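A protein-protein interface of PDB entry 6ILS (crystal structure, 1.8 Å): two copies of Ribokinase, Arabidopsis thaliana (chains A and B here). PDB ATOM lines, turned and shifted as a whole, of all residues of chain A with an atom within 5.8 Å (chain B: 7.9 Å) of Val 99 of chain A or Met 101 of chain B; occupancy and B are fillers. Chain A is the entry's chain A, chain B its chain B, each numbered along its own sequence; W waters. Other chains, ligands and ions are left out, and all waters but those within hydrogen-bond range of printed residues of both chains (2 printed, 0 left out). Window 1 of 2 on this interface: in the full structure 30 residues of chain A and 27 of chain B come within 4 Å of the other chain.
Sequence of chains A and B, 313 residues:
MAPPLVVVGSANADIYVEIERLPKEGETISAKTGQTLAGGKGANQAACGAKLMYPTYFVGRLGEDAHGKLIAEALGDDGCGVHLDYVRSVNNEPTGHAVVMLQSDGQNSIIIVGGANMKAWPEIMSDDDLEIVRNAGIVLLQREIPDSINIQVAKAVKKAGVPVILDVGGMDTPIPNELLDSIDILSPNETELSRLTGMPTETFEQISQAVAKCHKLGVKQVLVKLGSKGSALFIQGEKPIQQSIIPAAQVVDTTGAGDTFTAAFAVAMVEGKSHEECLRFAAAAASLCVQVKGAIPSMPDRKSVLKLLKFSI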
ATOM      1  N   ALA A  13     -16.275 -12.121 -19.515  1.00  0.00           N
ATOM      2  CA  ALA A  13     -16.077 -11.032 -18.572  1.00  0.00           C
ATOM      3  C   ALA A  13     -16.570 -11.518 -17.218  1.00  0.00           C
ATOM      4  O   ALA A  13     -17.716 -11.915 -17.087  1.00  0.00           O
ATOM      5  CB  ALA A  13     -16.825  -9.780 -19.005  1.00  0.00           C
ATOM      6  N   ILE A  15     -17.692 -10.559 -13.715  1.00  0.00           N
ATOM      7  CA  ILE A  15     -18.234  -9.395 -13.036  1.00  0.00           C
ATOM      8  C   ILE A  15     -18.410  -9.687 -11.551  1.00  0.00           C
ATOM      9  O   ILE A  15     -19.417 -10.250 -11.131  1.00  0.00           O
ATOM     10  CB  ILE A  15     -19.556  -8.986 -13.653  1.00  0.00           C
ATOM     11  CG1 ILE A  15     -19.377  -8.780 -15.157  1.00  0.00           C
ATOM     12  CG2 ILE A  15     -20.083  -7.706 -12.990  1.00  0.00           C
ATOM     13  CD1 ILE A  15     -20.650  -8.788 -15.917  1.00  0.00           C
ATOM     14  N   TYR A  16     -17.400  -9.314 -10.776  1.00  0.00           N
ATOM     15  CA  TYR A  16     -17.378  -9.524  -9.334  1.00  0.00           C
ATOM     16  C   TYR A  16     -18.026  -8.356  -8.605  1.00  0.00           C
ATOM     17  O   TYR A  16     -17.661  -7.202  -8.839  1.00  0.00           O
ATOM     18  CB  TYR A  16     -15.947  -9.675  -8.825  1.00  0.00           C
ATOM     19  CG  TYR A  16     -15.155 -10.842  -9.355  1.00  0.00           C
ATOM     20  CD1 TYR A  16     -15.212 -12.091  -8.735  1.00  0.00           C
ATOM     21  CD2 TYR A  16     -14.299 -10.687 -10.447  1.00  0.00           C
ATOM     22  CE1 TYR A  16     -14.462 -13.157  -9.211  1.00  0.00           C
ATOM     23  CE2 TYR A  16     -13.549 -11.744 -10.925  1.00  0.00           C
ATOM     24  CZ  TYR A  16     -13.629 -12.972 -10.303  1.00  0.00           C
ATOM     25  OH  TYR A  16     -12.872 -14.012 -10.789  1.00  0.00           O
ATOM     26  N   VAL A  17     -18.974  -8.644  -7.721  1.00  0.00           N
ATOM     27  CA  VAL A  17     -19.519  -7.609  -6.851  1.00  0.00           C
ATOM     28  C   VAL A  17     -19.462  -8.074  -5.395  1.00  0.00           C
ATOM     29  O   VAL A  17     -19.801  -9.218  -5.084  1.00  0.00           O
ATOM     30  CB  VAL A  17     -20.973  -7.233  -7.228  1.00  0.00           C
ATOM     31  CG1 VAL A  17     -21.011  -6.499  -8.571  1.00  0.00           C
ATOM     32  CG2 VAL A  17     -21.864  -8.458  -7.250  1.00  0.00           C
ATOM     33  N   PRO A  23     -29.821  -9.850  -2.793  1.00  0.00           N
ATOM     34  CA  PRO A  23     -31.073  -9.085  -2.841  1.00  0.00           C
ATOM     35  C   PRO A  23     -32.320  -9.968  -2.832  1.00  0.00           C
ATOM     36  O   PRO A  23     -32.216 -11.191  -2.725  1.00  0.00           O
ATOM     37  CB  PRO A  23     -30.965  -8.324  -4.164  1.00  0.00           C
ATOM     38  CG  PRO A  23     -30.112  -9.186  -5.009  1.00  0.00           C
ATOM     39  CD  PRO A  23     -29.114  -9.824  -4.086  1.00  0.00           C
ATOM     40  N   HIS A  97     -20.395 -13.959 -20.125  1.00  0.00           N
ATOM     41  CA  HIS A  97     -20.028 -13.367 -18.844  1.00  0.00           C
ATOM     42  C   HIS A  97     -20.600 -14.095 -17.632  1.00  0.00           C
ATOM     43  O   HIS A  97     -21.522 -14.905 -17.728  1.00  0.00           O
ATOM     44  CB  HIS A  97     -20.436 -11.886 -18.788  1.00  0.00           C
ATOM     45  CG  HIS A  97     -21.853 -11.611 -19.191  1.00  0.00           C
ATOM     46  ND1 HIS A  97     -22.318 -11.824 -20.471  1.00  0.00           N
ATOM     47  CD2 HIS A  97     -22.886 -11.073 -18.502  1.00  0.00           C
ATOM     48  CE1 HIS A  97     -23.589 -11.466 -20.543  1.00  0.00           C
ATOM     49  NE2 HIS A  97     -23.958 -11.007 -19.361  1.00  0.00           N
ATOM     50  N   ALA A  98     -20.006 -13.795 -16.487  1.00  0.00           N
ATOM     51  CA  ALA A  98     -20.400 -14.387 -15.219  1.00  0.00           C
ATOM     52  C   ALA A  98     -20.577 -13.285 -14.179  1.00  0.00           C
ATOM     53  O   ALA A  98     -19.677 -12.460 -13.986  1.00  0.00           O
ATOM     54  CB  ALA A  98     -19.360 -15.387 -14.756  1.00  0.00           C
ATOM     55  N   VAL A  99     -21.736 -13.261 -13.529  1.00  0.00           N
ATOM     56  CA  VAL A  99     -21.946 -12.364 -12.395  1.00  0.00           C
ATOM     57  C   VAL A  99     -21.609 -13.117 -11.105  1.00  0.00           C
ATOM     58  O   VAL A  99     -22.314 -14.049 -10.715  1.00  0.00           O
ATOM     59  CB  VAL A  99     -23.388 -11.829 -12.341  1.00  0.00           C
ATOM     60  CG1 VAL A  99     -23.581 -10.944 -11.111  1.00  0.00           C
ATOM     61  CG2 VAL A  99     -23.732 -11.063 -13.625  1.00  0.00           C
ATOM     62  N   VAL A 100     -20.514 -12.728 -10.463  1.00  0.00           N
ATOM     63  CA  VAL A 100     -20.089 -13.365  -9.226  1.00  0.00           C
ATOM     64  C   VAL A 100     -20.415 -12.487  -8.021  1.00  0.00           C
ATOM     65  O   VAL A 100     -19.900 -11.377  -7.898  1.00  0.00           O
ATOM     66  CB  VAL A 100     -18.579 -13.660  -9.231  1.00  0.00           C
ATOM     67  CG1 VAL A 100     -18.182 -14.363  -7.952  1.00  0.00           C
ATOM     68  CG2 VAL A 100     -18.195 -14.490 -10.449  1.00  0.00           C
ATOM     69  N   MET A 101     -21.259 -12.986  -7.125  1.00  0.00           N
ATOM     70  CA  MET A 101     -21.676 -12.203  -5.966  1.00  0.00           C
ATOM     71  C   MET A 101     -21.050 -12.689  -4.663  1.00  0.00           C
ATOM     72  O   MET A 101     -21.662 -13.449  -3.910  1.00  0.00           O
ATOM     73  CB  MET A 101     -23.194 -12.211  -5.858  1.00  0.00           C
ATOM     74  CG  MET A 101     -23.844 -11.453  -6.978  1.00  0.00           C
ATOM     75  SD  MET A 101     -25.565 -11.877  -7.197  1.00  0.00           S
ATOM     76  CE  MET A 101     -25.425 -13.532  -7.870  1.00  0.00           C
ATOM     77  N   SER A 109     -22.487 -16.564  -4.982  1.00  0.00           N
ATOM     78  CA  SER A 109     -23.629 -16.861  -5.835  1.00  0.00           C
ATOM     79  C   SER A 109     -23.275 -16.429  -7.252  1.00  0.00           C
ATOM     80  O   SER A 109     -22.772 -15.321  -7.453  1.00  0.00           O
ATOM     81  CB  SER A 109     -24.889 -16.150  -5.343  1.00  0.00           C
ATOM     82  OG  SER A 109     -25.120 -16.433  -3.973  1.00  0.00           O
ATOM     83  N   ILE A 110     -23.513 -17.299  -8.231  1.00  0.00           N
ATOM     84  CA  ILE A 110     -23.064 -17.025  -9.594  1.00  0.00           C
ATOM     85  C   ILE A 110     -24.158 -17.179 -10.651  1.00  0.00           C
ATOM     86  O   ILE A 110     -24.911 -18.155 -10.655  1.00  0.00           O
ATOM     87  CB  ILE A 110     -21.878 -17.933  -9.979  1.00  0.00           C
ATOM     88  CG1 ILE A 110     -20.759 -17.805  -8.950  1.00  0.00           C
ATOM     89  CG2 ILE A 110     -21.353 -17.571 -11.364  1.00  0.00           C
ATOM     90  CD1 ILE A 110     -19.519 -18.610  -9.275  1.00  0.00           C
ATOM     91  N   ILE A 111     -24.250 -16.187 -11.532  1.00  0.00           N
ATOM     92  CA  ILE A 111     -25.044 -16.301 -12.745  1.00  0.00           C
ATOM     93  C   ILE A 111     -24.093 -16.399 -13.931  1.00  0.00           C
ATOM     94  O   ILE A 111     -23.274 -15.507 -14.149  1.00  0.00           O
ATOM     95  CB  ILE A 111     -25.981 -15.104 -12.942  1.00  0.00           C
ATOM     96  CG1 ILE A 111     -26.834 -14.872 -11.701  1.00  0.00           C
ATOM     97  CG2 ILE A 111     -26.857 -15.302 -14.167  1.00  0.00           C
ATOM     98  CD1 ILE A 111     -27.923 -13.856 -11.918  1.00  0.00           C
ATOM     99  N   ILE A 112     -24.188 -17.480 -14.693  1.00  0.00           N
ATOM    100  CA  ILE A 112     -23.347 -17.636 -15.867  1.00  0.00           C
ATOM    101  C   ILE A 112     -24.152 -17.398 -17.140  1.00  0.00           C
ATOM    102  O   ILE A 112     -25.218 -17.987 -17.327  1.00  0.00           O
ATOM    103  CB  ILE A 112     -22.701 -19.027 -15.911  1.00  0.00           C
ATOM    104  CG1 ILE A 112     -21.866 -19.253 -14.650  1.00  0.00           C
ATOM    105  CG2 ILE A 112     -21.825 -19.166 -17.139  1.00  0.00           C
ATOM    106  CD1 ILE A 112     -21.152 -20.576 -14.633  1.00  0.00           C
ATOM    107  N   ILE B  15     -25.908  -3.933 -16.701  1.00  0.00           N
ATOM    108  CA  ILE B  15     -25.690  -5.342 -17.030  1.00  0.00           C
ATOM    109  C   ILE B  15     -26.967  -6.155 -16.792  1.00  0.00           C
ATOM    110  O   ILE B  15     -27.249  -6.563 -15.669  1.00  0.00           O
ATOM    111  CB  ILE B  15     -24.564  -5.974 -16.199  1.00  0.00           C
ATOM    112  CG1 ILE B  15     -23.318  -5.076 -16.137  1.00  0.00           C
ATOM    113  CG2 ILE B  15     -24.200  -7.340 -16.771  1.00  0.00           C
ATOM    114  CD1 ILE B  15     -22.544  -5.044 -17.393  1.00  0.00           C
ATOM    115  N   TYR B  16     -27.726  -6.377 -17.855  1.00  0.00           N
ATOM    116  CA  TYR B  16     -28.982  -7.120 -17.785  1.00  0.00           C
ATOM    117  C   TYR B  16     -28.772  -8.596 -18.015  1.00  0.00           C
ATOM    118  O   TYR B  16     -28.200  -8.979 -19.030  1.00  0.00           O
ATOM    119  CB  TYR B  16     -29.963  -6.598 -18.827  1.00  0.00           C
ATOM    120  CG  TYR B  16     -30.371  -5.175 -18.583  1.00  0.00           C
ATOM    121  CD1 TYR B  16     -31.345  -4.870 -17.647  1.00  0.00           C
ATOM    122  CD2 TYR B  16     -29.776  -4.134 -19.280  1.00  0.00           C
ATOM    123  CE1 TYR B  16     -31.723  -3.570 -17.411  1.00  0.00           C
ATOM    124  CE2 TYR B  16     -30.145  -2.826 -19.056  1.00  0.00           C
ATOM    125  CZ  TYR B  16     -31.120  -2.549 -18.116  1.00  0.00           C
ATOM    126  OH  TYR B  16     -31.495  -1.243 -17.883  1.00  0.00           O
ATOM    127  N   VAL B  17     -29.237  -9.422 -17.083  1.00  0.00           N
ATOM    128  CA  VAL B  17     -29.247 -10.860 -17.302  1.00  0.00           C
ATOM    129  C   VAL B  17     -30.669 -11.403 -17.131  1.00  0.00           C
ATOM    130  O   VAL B  17     -31.346 -11.124 -16.134  1.00  0.00           O
ATOM    131  CB  VAL B  17     -28.262 -11.604 -16.363  1.00  0.00           C
ATOM    132  CG1 VAL B  17     -26.822 -11.169 -16.650  1.00  0.00           C
ATOM    133  CG2 VAL B  17     -28.604 -11.376 -14.896  1.00  0.00           C
ATOM    134  N   GLU B  18     -31.129 -12.144 -18.136  1.00  0.00           N
ATOM    135  CA  GLU B  18     -32.430 -12.804 -18.076  1.00  0.00           C
ATOM    136  C   GLU B  18     -32.310 -14.156 -17.378  1.00  0.00           C
ATOM    137  O   GLU B  18     -31.629 -15.059 -17.871  1.00  0.00           O
ATOM    138  CB  GLU B  18     -33.002 -12.989 -19.475  1.00  0.00           C
ATOM    139  CG  GLU B  18     -33.563 -11.728 -20.085  1.00  0.00           C
ATOM    140  CD  GLU B  18     -34.053 -11.953 -21.499  1.00  0.00           C
ATOM    141  OE1 GLU B  18     -34.531 -13.076 -21.783  1.00  0.00           O
ATOM    142  OE2 GLU B  18     -33.964 -11.012 -22.326  1.00  0.00           O
ATOM    143  N   ILE B  19     -32.965 -14.296 -16.230  1.00  0.00           N
ATOM    144  CA  ILE B  19     -32.973 -15.563 -15.509  1.00  0.00           C
ATOM    145  C   ILE B  19     -34.409 -16.029 -15.253  1.00  0.00           C
ATOM    146  O   ILE B  19     -35.367 -15.296 -15.522  1.00  0.00           O
ATOM    147  CB  ILE B  19     -32.211 -15.459 -14.168  1.00  0.00           C
ATOM    148  CG1 ILE B  19     -32.879 -14.439 -13.242  1.00  0.00           C
ATOM    149  CG2 ILE B  19     -30.760 -15.074 -14.405  1.00  0.00           C
ATOM    150  CD1 ILE B  19     -32.094 -14.165 -11.970  1.00  0.00           C
ATOM    151  N   ARG B  21     -35.273 -17.585 -12.041  1.00  0.00           N
ATOM    152  CA  ARG B  21     -35.377 -17.174 -10.649  1.00  0.00           C
ATOM    153  C   ARG B  21     -34.025 -16.693 -10.137  1.00  0.00           C
ATOM    154  O   ARG B  21     -32.982 -17.083 -10.662  1.00  0.00           O
ATOM    155  CB  ARG B  21     -35.873 -18.334  -9.788  1.00  0.00           C
ATOM    156  CG  ARG B  21     -34.967 -19.556  -9.841  1.00  0.00           C
ATOM    157  CD  ARG B  21     -34.719 -20.127  -8.453  1.00  0.00           C
ATOM    158  NE  ARG B  21     -34.090 -21.445  -8.506  1.00  0.00           N
ATOM    159  CZ  ARG B  21     -32.779 -21.655  -8.437  1.00  0.00           C
ATOM    160  NH1 ARG B  21     -31.947 -20.630  -8.311  1.00  0.00           N
ATOM    161  NH2 ARG B  21     -32.298 -22.890  -8.494  1.00  0.00           N
ATOM    162  N   LEU B  22     -34.041 -15.850  -9.110  1.00  0.00           N
ATOM    163  CA  LEU B  22     -32.807 -15.456  -8.443  1.00  0.00           C
ATOM    164  C   LEU B  22     -32.120 -16.692  -7.854  1.00  0.00           C
ATOM    165  O   LEU B  22     -32.788 -17.598  -7.357  1.00  0.00           O
ATOM    166  CB  LEU B  22     -33.091 -14.419  -7.352  1.00  0.00           C
ATOM    167  N   PRO B  23     -30.781 -16.743  -7.927  1.00  0.00           N
ATOM    168  CA  PRO B  23     -30.048 -17.878  -7.358  1.00  0.00           C
ATOM    169  C   PRO B  23     -30.013 -17.817  -5.838  1.00  0.00           C
ATOM    170  O   PRO B  23     -30.389 -16.795  -5.258  1.00  0.00           O
ATOM    171  CB  PRO B  23     -28.644 -17.714  -7.938  1.00  0.00           C
ATOM    172  CG  PRO B  23     -28.509 -16.243  -8.128  1.00  0.00           C
ATOM    173  CD  PRO B  23     -29.875 -15.759  -8.545  1.00  0.00           C
ATOM    174  N   GLU B  27     -25.084 -21.165  -4.676  1.00  0.00           N
ATOM    175  CA  GLU B  27     -25.602 -21.779  -5.900  1.00  0.00           C
ATOM    176  C   GLU B  27     -25.220 -21.051  -7.195  1.00  0.00           C
ATOM    177  O   GLU B  27     -25.350 -19.828  -7.302  1.00  0.00           O
ATOM    178  CB  GLU B  27     -27.128 -21.882  -5.831  1.00  0.00           C
ATOM    179  CG  GLU B  27     -27.742 -22.655  -6.983  1.00  0.00           C
ATOM    180  CD  GLU B  27     -29.201 -22.314  -7.194  1.00  0.00           C
ATOM    181  OE1 GLU B  27     -29.663 -21.306  -6.618  1.00  0.00           O
ATOM    182  OE2 GLU B  27     -29.883 -23.052  -7.939  1.00  0.00           O
ATOM    183  N   THR B  28     -24.764 -21.828  -8.177  1.00  0.00           N
ATOM    184  CA  THR B  28     -24.516 -21.337  -9.529  1.00  0.00           C
ATOM    185  C   THR B  28     -25.710 -21.636 -10.433  1.00  0.00           C
ATOM    186  O   THR B  28     -26.187 -22.768 -10.474  1.00  0.00           O
ATOM    187  CB  THR B  28     -23.261 -21.984 -10.144  1.00  0.00           C
ATOM    188  OG1 THR B  28     -22.098 -21.601  -9.398  1.00  0.00           O
ATOM    189  CG2 THR B  28     -23.098 -21.560 -11.598  1.00  0.00           C
ATOM    190  N   ILE B  29     -26.202 -20.630 -11.149  1.00  0.00           N
ATOM    191  CA  ILE B  29     -27.244 -20.855 -12.146  1.00  0.00           C
ATOM    192  C   ILE B  29     -26.823 -20.340 -13.517  1.00  0.00           C
ATOM    193  O   ILE B  29     -25.763 -19.728 -13.666  1.00  0.00           O
ATOM    194  CB  ILE B  29     -28.560 -20.175 -11.766  1.00  0.00           C
ATOM    195  CG1 ILE B  29     -28.368 -18.659 -11.711  1.00  0.00           C
ATOM    196  CG2 ILE B  29     -29.073 -20.709 -10.445  1.00  0.00           C
ATOM    197  CD1 ILE B  29     -29.634 -17.882 -11.933  1.00  0.00           C
ATOM    198  N   ALA B  31     -28.121 -18.137 -17.080  1.00  0.00           N
ATOM    199  CA  ALA B  31     -29.073 -17.206 -17.659  1.00  0.00           C
ATOM    200  C   ALA B  31     -29.378 -17.597 -19.093  1.00  0.00           C
ATOM    201  O   ALA B  31     -28.582 -18.266 -19.748  1.00  0.00           O
ATOM    202  CB  ALA B  31     -28.532 -15.783 -17.599  1.00  0.00           C
ATOM    203  N   ALA B  98     -24.535  -1.452 -12.840  1.00  0.00           N
ATOM    204  CA  ALA B  98     -25.700  -2.029 -12.183  1.00  0.00           C
ATOM    205  C   ALA B  98     -26.000  -3.395 -12.788  1.00  0.00           C
ATOM    206  O   ALA B  98     -26.247  -3.504 -13.992  1.00  0.00           O
ATOM    207  CB  ALA B  98     -26.905  -1.110 -12.326  1.00  0.00           C
ATOM    208  N   VAL B  99     -25.954  -4.432 -11.961  1.00  0.00           N
ATOM    209  CA  VAL B  99     -26.360  -5.761 -12.398  1.00  0.00           C
ATOM    210  C   VAL B  99     -27.869  -5.903 -12.237  1.00  0.00           C
ATOM    211  O   VAL B  99     -28.378  -5.974 -11.117  1.00  0.00           O
ATOM    212  CB  VAL B  99     -25.647  -6.861 -11.610  1.00  0.00           C
ATOM    213  CG1 VAL B  99     -26.156  -8.235 -12.032  1.00  0.00           C
ATOM    214  CG2 VAL B  99     -24.143  -6.756 -11.818  1.00  0.00           C
ATOM    215  N   VAL B 100     -28.579  -5.926 -13.358  1.00  0.00           N
ATOM    216  CA  VAL B 100     -30.031  -5.992 -13.333  1.00  0.00           C
ATOM    217  C   VAL B 100     -30.514  -7.403 -13.682  1.00  0.00           C
ATOM    218  O   VAL B 100     -30.525  -7.797 -14.850  1.00  0.00           O
ATOM    219  CB  VAL B 100     -30.649  -4.970 -14.304  1.00  0.00           C
ATOM    220  CG1 VAL B 100     -32.164  -4.956 -14.172  1.00  0.00           C
ATOM    221  CG2 VAL B 100     -30.072  -3.587 -14.044  1.00  0.00           C
ATOM    222  N   MET B 101     -30.901  -8.160 -12.657  1.00  0.00           N
ATOM    223  CA  MET B 101     -31.385  -9.523 -12.843  1.00  0.00           C
ATOM    224  C   MET B 101     -32.886  -9.580 -13.109  1.00  0.00           C
ATOM    225  O   MET B 101     -33.695  -9.539 -12.178  1.00  0.00           O
ATOM    226  CB  MET B 101     -31.043 -10.370 -11.623  1.00  0.00           C
ATOM    227  CG  MET B 101     -29.562 -10.556 -11.444  1.00  0.00           C
ATOM    228  SD  MET B 101     -29.081 -10.782  -9.737  1.00  0.00           S
ATOM    229  CE  MET B 101     -27.322 -11.018  -9.928  1.00  0.00           C
ATOM    230  N   LEU B 102     -33.245  -9.676 -14.386  1.00  0.00           N
ATOM    231  CA  LEU B 102     -34.634  -9.825 -14.800  1.00  0.00           C
ATOM    232  C   LEU B 102     -35.124 -11.259 -14.585  1.00  0.00           C
ATOM    233  O   LEU B 102     -34.458 -12.221 -14.976  1.00  0.00           O
ATOM    234  CB  LEU B 102     -34.799  -9.433 -16.270  1.00  0.00           C
ATOM    235  CG  LEU B 102     -34.113  -8.155 -16.756  1.00  0.00           C
ATOM    236  CD1 LEU B 102     -34.243  -8.024 -18.266  1.00  0.00           C
ATOM    237  CD2 LEU B 102     -34.709  -6.942 -16.075  1.00  0.00           C
ATOM    238  N   GLN B 103     -36.287 -11.404 -13.959  1.00  0.00           N
ATOM    239  CA  GLN B 103     -36.876 -12.727 -13.771  1.00  0.00           C
ATOM    240  C   GLN B 103     -38.002 -12.966 -14.766  1.00  0.00           C
ATOM    241  O   GLN B 103     -38.465 -12.034 -15.427  1.00  0.00           O
ATOM    242  CB  GLN B 103     -37.393 -12.897 -12.346  1.00  0.00           C
ATOM    243  CG  GLN B 103     -36.309 -13.218 -11.339  1.00  0.00           C
ATOM    244  CD  GLN B 103     -36.333 -12.279 -10.152  1.00  0.00           C
ATOM    245  OE1 GLN B 103     -37.045 -11.272 -10.154  1.00  0.00           O
ATOM    246  NE2 GLN B 103     -35.553 -12.605  -9.124  1.00  0.00           N
ATOM    247  N   SER B 104     -38.437 -14.218 -14.870  1.00  0.00           N
ATOM    248  CA  SER B 104     -39.478 -14.587 -15.825  1.00  0.00           C
ATOM    249  C   SER B 104     -40.869 -14.105 -15.396  1.00  0.00           C
ATOM    250  O   SER B 104     -41.730 -13.853 -16.243  1.00  0.00           O
ATOM    251  CB  SER B 104     -39.493 -16.101 -16.033  1.00  0.00           C
ATOM    252  OG  SER B 104     -40.110 -16.429 -17.266  1.00  0.00           O
ATOM    253  N   ASP B 105     -41.083 -13.971 -14.088  1.00  0.00           N
ATOM    254  CA  ASP B 105     -42.366 -13.502 -13.570  1.00  0.00           C
ATOM    255  C   ASP B 105     -42.608 -12.029 -13.905  1.00  0.00           C
ATOM    256  O   ASP B 105     -43.703 -11.656 -14.332  1.00  0.00           O
ATOM    257  CB  ASP B 105     -42.458 -13.733 -12.055  1.00  0.00           C
ATOM    258  CG  ASP B 105     -41.220 -13.276 -11.308  1.00  0.00           C
ATOM    259  OD1 ASP B 105     -40.744 -12.149 -11.557  1.00  0.00           O
ATOM    260  OD2 ASP B 105     -40.722 -14.051 -10.463  1.00  0.00           O
ATOM    261  N   GLY B 106     -41.584 -11.199 -13.723  1.00  0.00           N
ATOM    262  CA  GLY B 106     -41.684  -9.791 -14.068  1.00  0.00           C
ATOM    263  C   GLY B 106     -40.923  -8.875 -13.133  1.00  0.00           C
ATOM    264  O   GLY B 106     -40.700  -7.704 -13.453  1.00  0.00           O
ATOM    265  N   GLN B 107     -40.533  -9.410 -11.977  1.00  0.00           N
ATOM    266  CA  GLN B 107     -39.789  -8.644 -10.987  1.00  0.00           C
ATOM    267  C   GLN B 107     -38.343  -8.437 -11.422  1.00  0.00           C
ATOM    268  O   GLN B 107     -37.761  -9.253 -12.151  1.00  0.00           O
ATOM    269  CB  GLN B 107     -39.831  -9.333  -9.618  1.00  0.00           C
ATOM    270  N   ASN B 108     -37.766  -7.325 -10.981  1.00  0.00           N
ATOM    271  CA  ASN B 108     -36.340  -7.063 -11.192  1.00  0.00           C
ATOM    272  C   ASN B 108     -35.588  -6.948  -9.883  1.00  0.00           C
ATOM    273  O   ASN B 108     -36.022  -6.257  -8.963  1.00  0.00           O
ATOM    274  CB  ASN B 108     -36.105  -5.775 -11.979  1.00  0.00           C
ATOM    275  CG  ASN B 108     -36.867  -5.735 -13.268  1.00  0.00           C
ATOM    276  OD1 ASN B 108     -37.181  -6.776 -13.842  1.00  0.00           O
ATOM    277  ND2 ASN B 108     -37.191  -4.523 -13.733  1.00  0.00           N
ATOM    278  N   SER B 109     -34.426  -7.573  -9.831  1.00  0.00           N
ATOM    279  CA  SER B 109     -33.554  -7.432  -8.693  1.00  0.00           C
ATOM    280  C   SER B 109     -32.274  -6.750  -9.169  1.00  0.00           C
ATOM    281  O   SER B 109     -31.705  -7.131 -10.198  1.00  0.00           O
ATOM    282  CB  SER B 109     -33.273  -8.791  -8.058  1.00  0.00           C
ATOM    283  OG  SER B 109     -32.321  -8.664  -7.033  1.00  0.00           O
ATOM    284  N   ILE B 110     -31.827  -5.734  -8.432  1.00  0.00           N
ATOM    285  CA  ILE B 110     -30.714  -4.916  -8.898  1.00  0.00           C
ATOM    286  C   ILE B 110     -29.605  -4.756  -7.862  1.00  0.00           C
ATOM    287  O   ILE B 110     -29.873  -4.500  -6.689  1.00  0.00           O
ATOM    288  CB  ILE B 110     -31.211  -3.518  -9.339  1.00  0.00           C
ATOM    289  CG1 ILE B 110     -32.152  -3.662 -10.538  1.00  0.00           C
ATOM    290  CG2 ILE B 110     -30.033  -2.596  -9.680  1.00  0.00           C
ATOM    291  CD1 ILE B 110     -32.520  -2.371 -11.213  1.00  0.00           C
ATOM    292  N   ILE B 111     -28.361  -4.948  -8.308  1.00  0.00           N
ATOM    293  CA  ILE B 111     -27.170  -4.614  -7.527  1.00  0.00           C
ATOM    294  C   ILE B 111     -26.454  -3.433  -8.182  1.00  0.00           C
ATOM    295  O   ILE B 111     -26.076  -3.504  -9.356  1.00  0.00           O
ATOM    296  CB  ILE B 111     -26.193  -5.796  -7.415  1.00  0.00           C
ATOM    297  CG1 ILE B 111     -26.902  -7.040  -6.878  1.00  0.00           C
ATOM    298  CG2 ILE B 111     -25.008  -5.432  -6.535  1.00  0.00           C
ATOM    299  CD1 ILE B 111     -25.964  -8.193  -6.577  1.00  0.00           C
HETATM  300  O   HOH W   1     -26.002 -19.349 -19.901  1.00  0.00           O
HETATM  301  O   HOH W   2     -25.452  -9.082 -19.937  1.00  0.00           O
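Ile 15 of chain B touches Ile 15 of chain A (CG2 to CD1, 3.9 Å).
Pro 23 of chain A touches Ser 109 of chain B (CG to OG, 3.0 Å).
CA of Ser 109 of chain A touches O of Glu 27 of chain B, at 3.7 Å.
CA of Thr 28 of chain B touches O of Ile 110 of chain A, at 3.4 Å.
Ile 111 of chain A touches Val 17 of chain B (CD1 to CG2, 3.9 Å).
CD1 of Ile 112 of chain A touches CG2 of Thr 28 of chain B, 3.7 Å away.
The backbone carbonyl oxygen of Leu 102 of chain B is in hydrogen-bond range of the backbone NH of Ile 19 of chain B (2.8 Å).
NH2 of Arg 21 of chain B lies within salt-bridge range of OE2 of Glu 27 of chain B (2.5 Å).
The backbone NH (N) of Val 99 of chain B lies within hydrogen-bond range of the backbone carbonyl oxygen (O) of Ile 111 of chain B.
The backbone NH (N) of Ile 110 of chain A is in hydrogen-bond range of the backbone carbonyl oxygen (O) of Glu 27 of chain B, at 3.3 Å.
O of Ile 110 of chain A lies within hydrogen-bond range of N of Ile 29 of chain B (2.8 Å).
O of Ile 29 of chain B lies within hydrogen-bond range of N of Ile 112 of chain A (2.9 Å).
N of Ala 31 of chain B is in hydrogen-bond range of O of Ile 112 of chain A (2.9 Å).
Water W2 lies within hydrogen-bond range of a ring nitrogen (NE2) of His 97 of chain A (2.5 Å) and the backbone carbonyl oxygen (O) of Tyr 16 of chain B (2.9 Å).
Water W1 bridges the backbone carbonyl oxygen of Ala 31 of chain B (2.8 Å) and the backbone carbonyl oxygen of Ile 112 of chain A (3.0 Å).
Of chain B, only Val 99 and Met 101 come within 4 Å of Val 99 of chain A.
Met 101 of chain B touches just these residues of chain A: Val 99 (3.9 Å), Met 101 (3.4 Å) and Ile 111 (3.5 Å).
Printed residues of chain A within 4 Å of Ala 31 of chain B: Ile 111 and Ile 112.
Of the printed residues of chain B, His 97 of chain A touches Val 17 (3.9 Å).
Of the printed residues of chain A, Val 17 of chain B touches His 97 and Ile 111.
Pro 23 of chain B touches none of the printed residues of chain A.
The nearest residue of chain B that does not touch Val 99 of chain A is Val 17 of chain B (4.3 Å).
The nearest residue of chain A that does not touch Met 101 of chain B is Pro 23 of chain A (5.1 Å).
Of the 14 printed residues of chain A, 9 touch a printed residue of chain B.
Printed residues of chain A that touch a printed residue of chain B: Ile 15, Pro 23, His 97, Val 99, Met 101, Ser 109, Ile 110, Ile 111 and Ile 112.
Of the 26 printed residues of chain B, 11 touch a printed residue of chain A.
Hydrophobic or aromatic side chains of chain B that line the printed part of chain A: Ile 15, Val 17, Ile 19, Ile 29, Ala 31, Val 99, Met 101 and Ile 111.
Among the printed residues, 19 pairs touch across the chains.
Ile 15 of chain B touches its own counterpart, Ile 15 of chain A.
Pro 23 of chain A touches Ser 109 of chain B, but with the chains exchanged Ser 109 of chain A does not touch Pro 23 of chain B (4.6 Å).
Val 99 of chain A touches its own counterpart, Val 99 of chain B.
Met 101 of chain A touches its own counterpart, Met 101 of chain B.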
